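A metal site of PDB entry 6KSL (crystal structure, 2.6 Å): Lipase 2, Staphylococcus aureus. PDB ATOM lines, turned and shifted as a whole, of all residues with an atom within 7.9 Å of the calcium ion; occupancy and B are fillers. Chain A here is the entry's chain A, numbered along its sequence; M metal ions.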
ATOM      1  N   LYS A  51       3.285 -13.392 -18.889  1.00  0.00           N
ATOM      2  CA  LYS A  51       4.446 -14.234 -18.907  1.00  0.00           C
ATOM      3  C   LYS A  51       5.595 -13.657 -19.745  1.00  0.00           C
ATOM      4  O   LYS A  51       6.760 -13.923 -19.435  1.00  0.00           O
ATOM      5  CB  LYS A  51       4.074 -15.651 -19.347  1.00  0.00           C
ATOM      6  CG  LYS A  51       3.115 -16.294 -18.366  1.00  0.00           C
ATOM      7  CD  LYS A  51       2.990 -17.768 -18.611  1.00  0.00           C
ATOM      8  CE  LYS A  51       1.835 -18.300 -17.817  1.00  0.00           C
ATOM      9  NZ  LYS A  51       1.780 -19.759 -18.070  1.00  0.00           N
ATOM     10  N   VAL A 282       0.327 -30.086 -28.604  1.00  0.00           N
ATOM     11  CA  VAL A 282      -0.557 -31.181 -28.097  1.00  0.00           C
ATOM     12  C   VAL A 282      -0.655 -30.961 -26.637  1.00  0.00           C
ATOM     13  O   VAL A 282       0.317 -30.538 -25.993  1.00  0.00           O
ATOM     14  CB  VAL A 282      -0.021 -32.652 -28.095  1.00  0.00           C
ATOM     15  CG1 VAL A 282      -0.708 -33.585 -29.094  1.00  0.00           C
ATOM     16  CG2 VAL A 282       1.483 -32.766 -28.102  1.00  0.00           C
ATOM     17  N   SER A 283      -1.842 -31.252 -26.106  1.00  0.00           N
ATOM     18  CA  SER A 283      -2.133 -31.043 -24.704  1.00  0.00           C
ATOM     19  C   SER A 283      -3.205 -32.065 -24.306  1.00  0.00           C
ATOM     20  O   SER A 283      -4.025 -31.855 -23.393  1.00  0.00           O
ATOM     21  CB  SER A 283      -2.545 -29.573 -24.512  1.00  0.00           C
ATOM     22  OG  SER A 283      -3.161 -29.350 -23.274  1.00  0.00           O
ATOM     23  N   ASP A 295      -4.903 -32.967 -20.982  1.00  0.00           N
ATOM     24  CA  ASP A 295      -3.942 -33.052 -19.861  1.00  0.00           C
ATOM     25  C   ASP A 295      -4.336 -32.069 -18.763  1.00  0.00           C
ATOM     26  O   ASP A 295      -4.890 -30.997 -19.080  1.00  0.00           O
ATOM     27  CB  ASP A 295      -2.515 -32.667 -20.296  1.00  0.00           C
ATOM     28  CG  ASP A 295      -1.968 -33.522 -21.424  1.00  0.00           C
ATOM     29  OD1 ASP A 295      -2.555 -34.609 -21.693  1.00  0.00           O
ATOM     30  OD2 ASP A 295      -0.941 -33.085 -22.026  1.00  0.00           O
ATOM     31  N   LEU A 296      -4.022 -32.405 -17.499  1.00  0.00           N
ATOM     32  CA  LEU A 296      -4.053 -31.415 -16.436  1.00  0.00           C
ATOM     33  C   LEU A 296      -3.155 -30.307 -16.933  1.00  0.00           C
ATOM     34  O   LEU A 296      -2.034 -30.544 -17.497  1.00  0.00           O
ATOM     35  CB  LEU A 296      -3.531 -32.007 -15.111  1.00  0.00           C
ATOM     36  CG  LEU A 296      -4.556 -32.393 -14.030  1.00  0.00           C
ATOM     37  CD1 LEU A 296      -4.570 -31.434 -12.845  1.00  0.00           C
ATOM     38  CD2 LEU A 296      -5.988 -32.587 -14.566  1.00  0.00           C
ATOM     39  N   GLY A 297      -3.629 -29.076 -16.799  1.00  0.00           N
ATOM     40  CA  GLY A 297      -2.763 -27.983 -17.274  1.00  0.00           C
ATOM     41  C   GLY A 297      -3.190 -27.373 -18.579  1.00  0.00           C
ATOM     42  O   GLY A 297      -2.695 -26.328 -18.934  1.00  0.00           O
ATOM     43  N   THR A 298      -4.224 -27.960 -19.156  1.00  0.00           N
ATOM     44  CA  THR A 298      -4.867 -27.418 -20.326  1.00  0.00           C
ATOM     45  C   THR A 298      -5.836 -26.418 -19.738  1.00  0.00           C
ATOM     46  O   THR A 298      -6.550 -26.768 -18.813  1.00  0.00           O
ATOM     47  CB  THR A 298      -5.691 -28.484 -21.025  1.00  0.00           C
ATOM     48  OG1 THR A 298      -4.843 -29.260 -21.858  1.00  0.00           O
ATOM     49  CG2 THR A 298      -6.723 -27.850 -21.890  1.00  0.00           C
ATOM     50  N   PHE A 299      -5.855 -25.197 -20.240  1.00  0.00           N
ATOM     51  CA  PHE A 299      -6.726 -24.151 -19.733  1.00  0.00           C
ATOM     52  C   PHE A 299      -8.164 -24.607 -19.616  1.00  0.00           C
ATOM     53  O   PHE A 299      -8.816 -24.868 -20.591  1.00  0.00           O
ATOM     54  CB  PHE A 299      -6.648 -22.917 -20.599  1.00  0.00           C
ATOM     55  CG  PHE A 299      -7.286 -21.728 -19.992  1.00  0.00           C
ATOM     56  CD1 PHE A 299      -6.934 -21.312 -18.738  1.00  0.00           C
ATOM     57  CD2 PHE A 299      -8.261 -21.042 -20.669  1.00  0.00           C
ATOM     58  CE1 PHE A 299      -7.524 -20.220 -18.164  1.00  0.00           C
ATOM     59  CE2 PHE A 299      -8.861 -19.941 -20.112  1.00  0.00           C
ATOM     60  CZ  PHE A 299      -8.493 -19.539 -18.852  1.00  0.00           C
ATOM     61  N   PHE A 300      -8.609 -24.737 -18.387  1.00  0.00           N
ATOM     62  CA  PHE A 300      -9.929 -25.235 -18.057  1.00  0.00           C
ATOM     63  C   PHE A 300     -11.094 -24.818 -18.909  1.00  0.00           C
ATOM     64  O   PHE A 300     -12.107 -25.494 -18.921  1.00  0.00           O
ATOM     65  CB  PHE A 300     -10.246 -25.008 -16.583  1.00  0.00           C
ATOM     66  CG  PHE A 300     -10.711 -23.630 -16.253  1.00  0.00           C
ATOM     67  CD1 PHE A 300      -9.827 -22.578 -16.249  1.00  0.00           C
ATOM     68  CD2 PHE A 300     -12.007 -23.401 -15.922  1.00  0.00           C
ATOM     69  CE1 PHE A 300     -10.247 -21.316 -15.938  1.00  0.00           C
ATOM     70  CE2 PHE A 300     -12.439 -22.132 -15.611  1.00  0.00           C
ATOM     71  CZ  PHE A 300     -11.560 -21.093 -15.623  1.00  0.00           C
ATOM     72  N   MET A 302     -11.146 -24.775 -22.150  1.00  0.00           N
ATOM     73  CA  MET A 302     -11.143 -25.567 -23.340  1.00  0.00           C
ATOM     74  C   MET A 302     -11.274 -27.023 -22.988  1.00  0.00           C
ATOM     75  O   MET A 302     -10.936 -27.880 -23.773  1.00  0.00           O
ATOM     76  CB  MET A 302      -9.836 -25.374 -24.084  1.00  0.00           C
ATOM     77  CG  MET A 302      -9.542 -23.943 -24.457  1.00  0.00           C
ATOM     78  SD  MET A 302      -7.830 -23.829 -24.911  1.00  0.00           S
ATOM     79  CE  MET A 302      -7.508 -25.516 -25.311  1.00  0.00           C
ATOM     80  N   ASP A 321      -4.837 -29.423 -29.067  1.00  0.00           N
ATOM     81  CA  ASP A 321      -4.249 -28.489 -28.113  1.00  0.00           C
ATOM     82  C   ASP A 321      -5.334 -27.892 -27.210  1.00  0.00           C
ATOM     83  O   ASP A 321      -5.131 -26.843 -26.605  1.00  0.00           O
ATOM     84  CB  ASP A 321      -3.505 -27.380 -28.845  1.00  0.00           C
ATOM     85  CG  ASP A 321      -4.465 -26.405 -29.615  1.00  0.00           C
ATOM     86  OD1 ASP A 321      -5.712 -26.581 -29.578  1.00  0.00           O
ATOM     87  OD2 ASP A 321      -3.960 -25.446 -30.246  1.00  0.00           O
ATOM     88  N   GLY A 360       2.922 -30.852 -24.552  1.00  0.00           N
ATOM     89  CA  GLY A 360       2.218 -30.143 -23.483  1.00  0.00           C
ATOM     90  C   GLY A 360       1.974 -28.624 -23.631  1.00  0.00           C
ATOM     91  O   GLY A 360       1.829 -27.945 -22.644  1.00  0.00           O
ATOM     92  N   TRP A 361       1.961 -28.079 -24.841  1.00  0.00           N
ATOM     93  CA  TRP A 361       1.541 -26.693 -25.011  1.00  0.00           C
ATOM     94  C   TRP A 361       0.095 -26.733 -25.490  1.00  0.00           C
ATOM     95  O   TRP A 361      -0.194 -27.351 -26.522  1.00  0.00           O
ATOM     96  CB  TRP A 361       2.364 -26.030 -26.105  1.00  0.00           C
ATOM     97  CG  TRP A 361       3.685 -25.582 -25.686  1.00  0.00           C
ATOM     98  CD1 TRP A 361       4.603 -26.301 -24.978  1.00  0.00           C
ATOM     99  CD2 TRP A 361       4.300 -24.306 -25.957  1.00  0.00           C
ATOM    100  NE1 TRP A 361       5.743 -25.558 -24.786  1.00  0.00           N
ATOM    101  CE2 TRP A 361       5.590 -24.326 -25.355  1.00  0.00           C
ATOM    102  CE3 TRP A 361       3.876 -23.155 -26.660  1.00  0.00           C
ATOM    103  CZ2 TRP A 361       6.492 -23.231 -25.416  1.00  0.00           C
ATOM    104  CZ3 TRP A 361       4.775 -22.066 -26.729  1.00  0.00           C
ATOM    105  CH2 TRP A 361       6.088 -22.102 -26.109  1.00  0.00           C
ATOM    106  N   ASP A 362      -0.817 -26.094 -24.753  1.00  0.00           N
ATOM    107  CA  ASP A 362      -2.177 -25.963 -25.221  1.00  0.00           C
ATOM    108  C   ASP A 362      -2.327 -24.725 -26.094  1.00  0.00           C
ATOM    109  O   ASP A 362      -1.358 -23.932 -26.272  1.00  0.00           O
ATOM    110  CB  ASP A 362      -3.217 -26.027 -24.094  1.00  0.00           C
ATOM    111  CG  ASP A 362      -3.265 -24.791 -23.236  1.00  0.00           C
ATOM    112  OD1 ASP A 362      -3.097 -23.637 -23.722  1.00  0.00           O
ATOM    113  OD2 ASP A 362      -3.487 -25.013 -21.998  1.00  0.00           O
ATOM    114  N   HIS A 363      -3.543 -24.567 -26.629  1.00  0.00           N
ATOM    115  CA  HIS A 363      -3.837 -23.530 -27.600  1.00  0.00           C
ATOM    116  C   HIS A 363      -3.372 -22.134 -27.162  1.00  0.00           C
ATOM    117  O   HIS A 363      -2.932 -21.292 -27.955  1.00  0.00           O
ATOM    118  CB  HIS A 363      -5.319 -23.529 -27.879  1.00  0.00           C
ATOM    119  CG  HIS A 363      -5.703 -22.676 -29.044  1.00  0.00           C
ATOM    120  ND1 HIS A 363      -5.462 -23.053 -30.354  1.00  0.00           N
ATOM    121  CD2 HIS A 363      -6.309 -21.460 -29.103  1.00  0.00           C
ATOM    122  CE1 HIS A 363      -5.919 -22.122 -31.166  1.00  0.00           C
ATOM    123  NE2 HIS A 363      -6.428 -21.137 -30.434  1.00  0.00           N
ATOM    124  N   VAL A 364      -3.440 -21.919 -25.878  1.00  0.00           N
ATOM    125  CA  VAL A 364      -3.438 -20.588 -25.380  1.00  0.00           C
ATOM    126  C   VAL A 364      -2.077 -20.377 -24.678  1.00  0.00           C
ATOM    127  O   VAL A 364      -1.682 -19.230 -24.391  1.00  0.00           O
ATOM    128  CB  VAL A 364      -4.693 -20.494 -24.534  1.00  0.00           C
ATOM    129  CG1 VAL A 364      -4.386 -20.536 -23.049  1.00  0.00           C
ATOM    130  CG2 VAL A 364      -5.553 -19.344 -24.925  1.00  0.00           C
ATOM    131  N   ASP A 365      -1.338 -21.488 -24.484  1.00  0.00           N
ATOM    132  CA  ASP A 365       0.027 -21.418 -23.975  1.00  0.00           C
ATOM    133  C   ASP A 365       0.905 -20.649 -24.934  1.00  0.00           C
ATOM    134  O   ASP A 365       1.810 -20.001 -24.490  1.00  0.00           O
ATOM    135  CB  ASP A 365       0.634 -22.805 -23.762  1.00  0.00           C
ATOM    136  CG  ASP A 365       0.034 -23.577 -22.542  1.00  0.00           C
ATOM    137  OD1 ASP A 365      -0.257 -22.961 -21.486  1.00  0.00           O
ATOM    138  OD2 ASP A 365      -0.107 -24.839 -22.592  1.00  0.00           O
ATOM    139  N   PHE A 366       0.644 -20.733 -26.249  1.00  0.00           N
ATOM    140  CA  PHE A 366       1.388 -19.985 -27.265  1.00  0.00           C
ATOM    141  C   PHE A 366       1.332 -18.469 -27.083  1.00  0.00           C
ATOM    142  O   PHE A 366       2.174 -17.742 -27.584  1.00  0.00           O
ATOM    143  CB  PHE A 366       0.877 -20.306 -28.655  1.00  0.00           C
ATOM    144  CG  PHE A 366       1.296 -21.667 -29.151  1.00  0.00           C
ATOM    145  CD1 PHE A 366       2.562 -21.857 -29.748  1.00  0.00           C
ATOM    146  CD2 PHE A 366       0.431 -22.766 -29.061  1.00  0.00           C
ATOM    147  CE1 PHE A 366       2.946 -23.127 -30.210  1.00  0.00           C
ATOM    148  CE2 PHE A 366       0.809 -24.046 -29.515  1.00  0.00           C
ATOM    149  CZ  PHE A 366       2.075 -24.233 -30.087  1.00  0.00           C
ATOM    150  N   ASP A 370      -2.508 -18.472 -20.107  1.00  0.00           N
ATOM    151  CA  ASP A 370      -2.852 -19.484 -19.127  1.00  0.00           C
ATOM    152  C   ASP A 370      -2.159 -19.213 -17.771  1.00  0.00           C
ATOM    153  O   ASP A 370      -1.139 -19.847 -17.459  1.00  0.00           O
ATOM    154  CB  ASP A 370      -2.456 -20.836 -19.714  1.00  0.00           C
ATOM    155  CG  ASP A 370      -2.947 -22.002 -18.918  1.00  0.00           C
ATOM    156  OD1 ASP A 370      -3.557 -21.812 -17.824  1.00  0.00           O
ATOM    157  OD2 ASP A 370      -2.666 -23.131 -19.402  1.00  0.00           O
ATOM    158  N   PHE A 371      -2.703 -18.278 -16.991  1.00  0.00           N
ATOM    159  CA  PHE A 371      -2.156 -17.888 -15.639  1.00  0.00           C
ATOM    160  C   PHE A 371      -2.108 -19.063 -14.625  1.00  0.00           C
ATOM    161  O   PHE A 371      -1.218 -19.115 -13.790  1.00  0.00           O
ATOM    162  CB  PHE A 371      -2.901 -16.677 -15.039  1.00  0.00           C
ATOM    163  CG  PHE A 371      -4.375 -16.925 -14.820  1.00  0.00           C
ATOM    164  CD1 PHE A 371      -5.296 -16.863 -15.886  1.00  0.00           C
ATOM    165  CD2 PHE A 371      -4.840 -17.248 -13.543  1.00  0.00           C
ATOM    166  CE1 PHE A 371      -6.643 -17.112 -15.683  1.00  0.00           C
ATOM    167  CE2 PHE A 371      -6.196 -17.499 -13.336  1.00  0.00           C
ATOM    168  CZ  PHE A 371      -7.089 -17.446 -14.417  1.00  0.00           C
ATOM    169  N   LEU A 372      -3.051 -19.991 -14.754  1.00  0.00           N
ATOM    170  CA  LEU A 372      -3.021 -21.245 -14.025  1.00  0.00           C
ATOM    171  C   LEU A 372      -1.877 -22.233 -14.354  1.00  0.00           C
ATOM    172  O   LEU A 372      -1.620 -23.122 -13.547  1.00  0.00           O
ATOM    173  CB  LEU A 372      -4.377 -21.927 -14.179  1.00  0.00           C
ATOM    174  CG  LEU A 372      -5.506 -21.568 -13.198  1.00  0.00           C
ATOM    175  CD1 LEU A 372      -5.187 -20.425 -12.236  1.00  0.00           C
ATOM    176  CD2 LEU A 372      -6.808 -21.284 -13.917  1.00  0.00           C
ATOM    177  N   ASP A 373      -1.197 -22.131 -15.496  1.00  0.00           N
ATOM    178  CA  ASP A 373      -0.192 -23.164 -15.876  1.00  0.00           C
ATOM    179  C   ASP A 373       1.211 -22.758 -15.465  1.00  0.00           C
ATOM    180  O   ASP A 373       1.915 -22.145 -16.236  1.00  0.00           O
ATOM    181  CB  ASP A 373      -0.234 -23.510 -17.375  1.00  0.00           C
ATOM    182  CG  ASP A 373       0.525 -24.824 -17.720  1.00  0.00           C
ATOM    183  OD1 ASP A 373       1.170 -25.423 -16.833  1.00  0.00           O
ATOM    184  OD2 ASP A 373       0.469 -25.263 -18.925  1.00  0.00           O
ATOM    185  N   PHE A 374       1.608 -23.140 -14.257  1.00  0.00           N
ATOM    186  CA  PHE A 374       2.944 -22.807 -13.730  1.00  0.00           C
ATOM    187  C   PHE A 374       4.072 -23.565 -14.435  1.00  0.00           C
ATOM    188  O   PHE A 374       5.184 -23.105 -14.461  1.00  0.00           O
ATOM    189  CB  PHE A 374       2.988 -22.957 -12.180  1.00  0.00           C
ATOM    190  CG  PHE A 374       1.856 -22.189 -11.455  1.00  0.00           C
ATOM    191  CD1 PHE A 374       1.664 -20.776 -11.630  1.00  0.00           C
ATOM    192  CD2 PHE A 374       0.965 -22.848 -10.575  1.00  0.00           C
ATOM    193  CE1 PHE A 374       0.631 -20.082 -10.960  1.00  0.00           C
ATOM    194  CE2 PHE A 374      -0.078 -22.164  -9.933  1.00  0.00           C
ATOM    195  CZ  PHE A 374      -0.254 -20.803 -10.164  1.00  0.00           C
ATOM    196  N   LYS A 375       3.768 -24.707 -15.053  1.00  0.00           N
ATOM    197  CA  LYS A 375       4.734 -25.512 -15.837  1.00  0.00           C
ATOM    198  C   LYS A 375       5.174 -24.851 -17.181  1.00  0.00           C
ATOM    199  O   LYS A 375       6.186 -25.260 -17.761  1.00  0.00           O
ATOM    200  CB  LYS A 375       4.180 -26.937 -16.069  1.00  0.00           C
ATOM    201  CG  LYS A 375       5.159 -28.095 -15.906  1.00  0.00           C
ATOM    202  CD  LYS A 375       5.237 -28.982 -17.166  1.00  0.00           C
ATOM    203  CE  LYS A 375       6.436 -28.646 -18.110  1.00  0.00           C
ATOM    204  NZ  LYS A 375       7.189 -29.806 -18.674  1.00  0.00           N
ATOM    205  N   ARG A 376       4.417 -23.852 -17.673  1.00  0.00           N
ATOM    206  CA  ARG A 376       4.797 -23.092 -18.890  1.00  0.00           C
ATOM    207  C   ARG A 376       5.340 -21.718 -18.486  1.00  0.00           C
ATOM    208  O   ARG A 376       4.557 -20.739 -18.346  1.00  0.00           O
ATOM    209  CB  ARG A 376       3.623 -22.959 -19.874  1.00  0.00           C
ATOM    210  CG  ARG A 376       3.049 -24.288 -20.327  1.00  0.00           C
ATOM    211  CD  ARG A 376       3.654 -24.820 -21.588  1.00  0.00           C
ATOM    212  NE  ARG A 376       5.091 -25.071 -21.481  1.00  0.00           N
ATOM    213  CZ  ARG A 376       5.614 -26.209 -21.040  1.00  0.00           C
ATOM    214  NH1 ARG A 376       6.934 -26.366 -20.979  1.00  0.00           N
ATOM    215  NH2 ARG A 376       4.825 -27.205 -20.651  1.00  0.00           N
HETATM  216 CA    CA M   1      -1.498 -25.009 -20.724  1.00  0.00          CA
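The backbone NH of Phe 299 lies close to the side-chain carboxylate of Asp 362. The backbone NH (N) of Val 364 lies within hydrogen-bond range of the side-chain carboxylate (OD1) of Asp 362. The side-chain amino group (NZ) of Lys 51 sits at hydrogen-bond distance from the backbone carbonyl oxygen (O) of Asp 370 (3.0 Å). NZ of Lys 51 lies within hydrogen-bond range of O of Asp 373 (3.0 Å). The side-chain carboxylate (OD1) of Asp 373 is in hydrogen-bond range of the backbone NH (N) of Lys 375, at 3.2 Å.
Along chain A the residues within 4 Å of the calcium ion span positions 297 to 373.
The calcium ion is bound by OD2 of Asp 365 (2.3 Å), OD2 of Asp 362 (2.4 Å), OD1 of Asp 365 (2.5 Å), O of Gly 297 (2.5 Å), OD2 of Asp 370 (2.6 Å) and OD2 of Asp 373 (2.7 Å).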
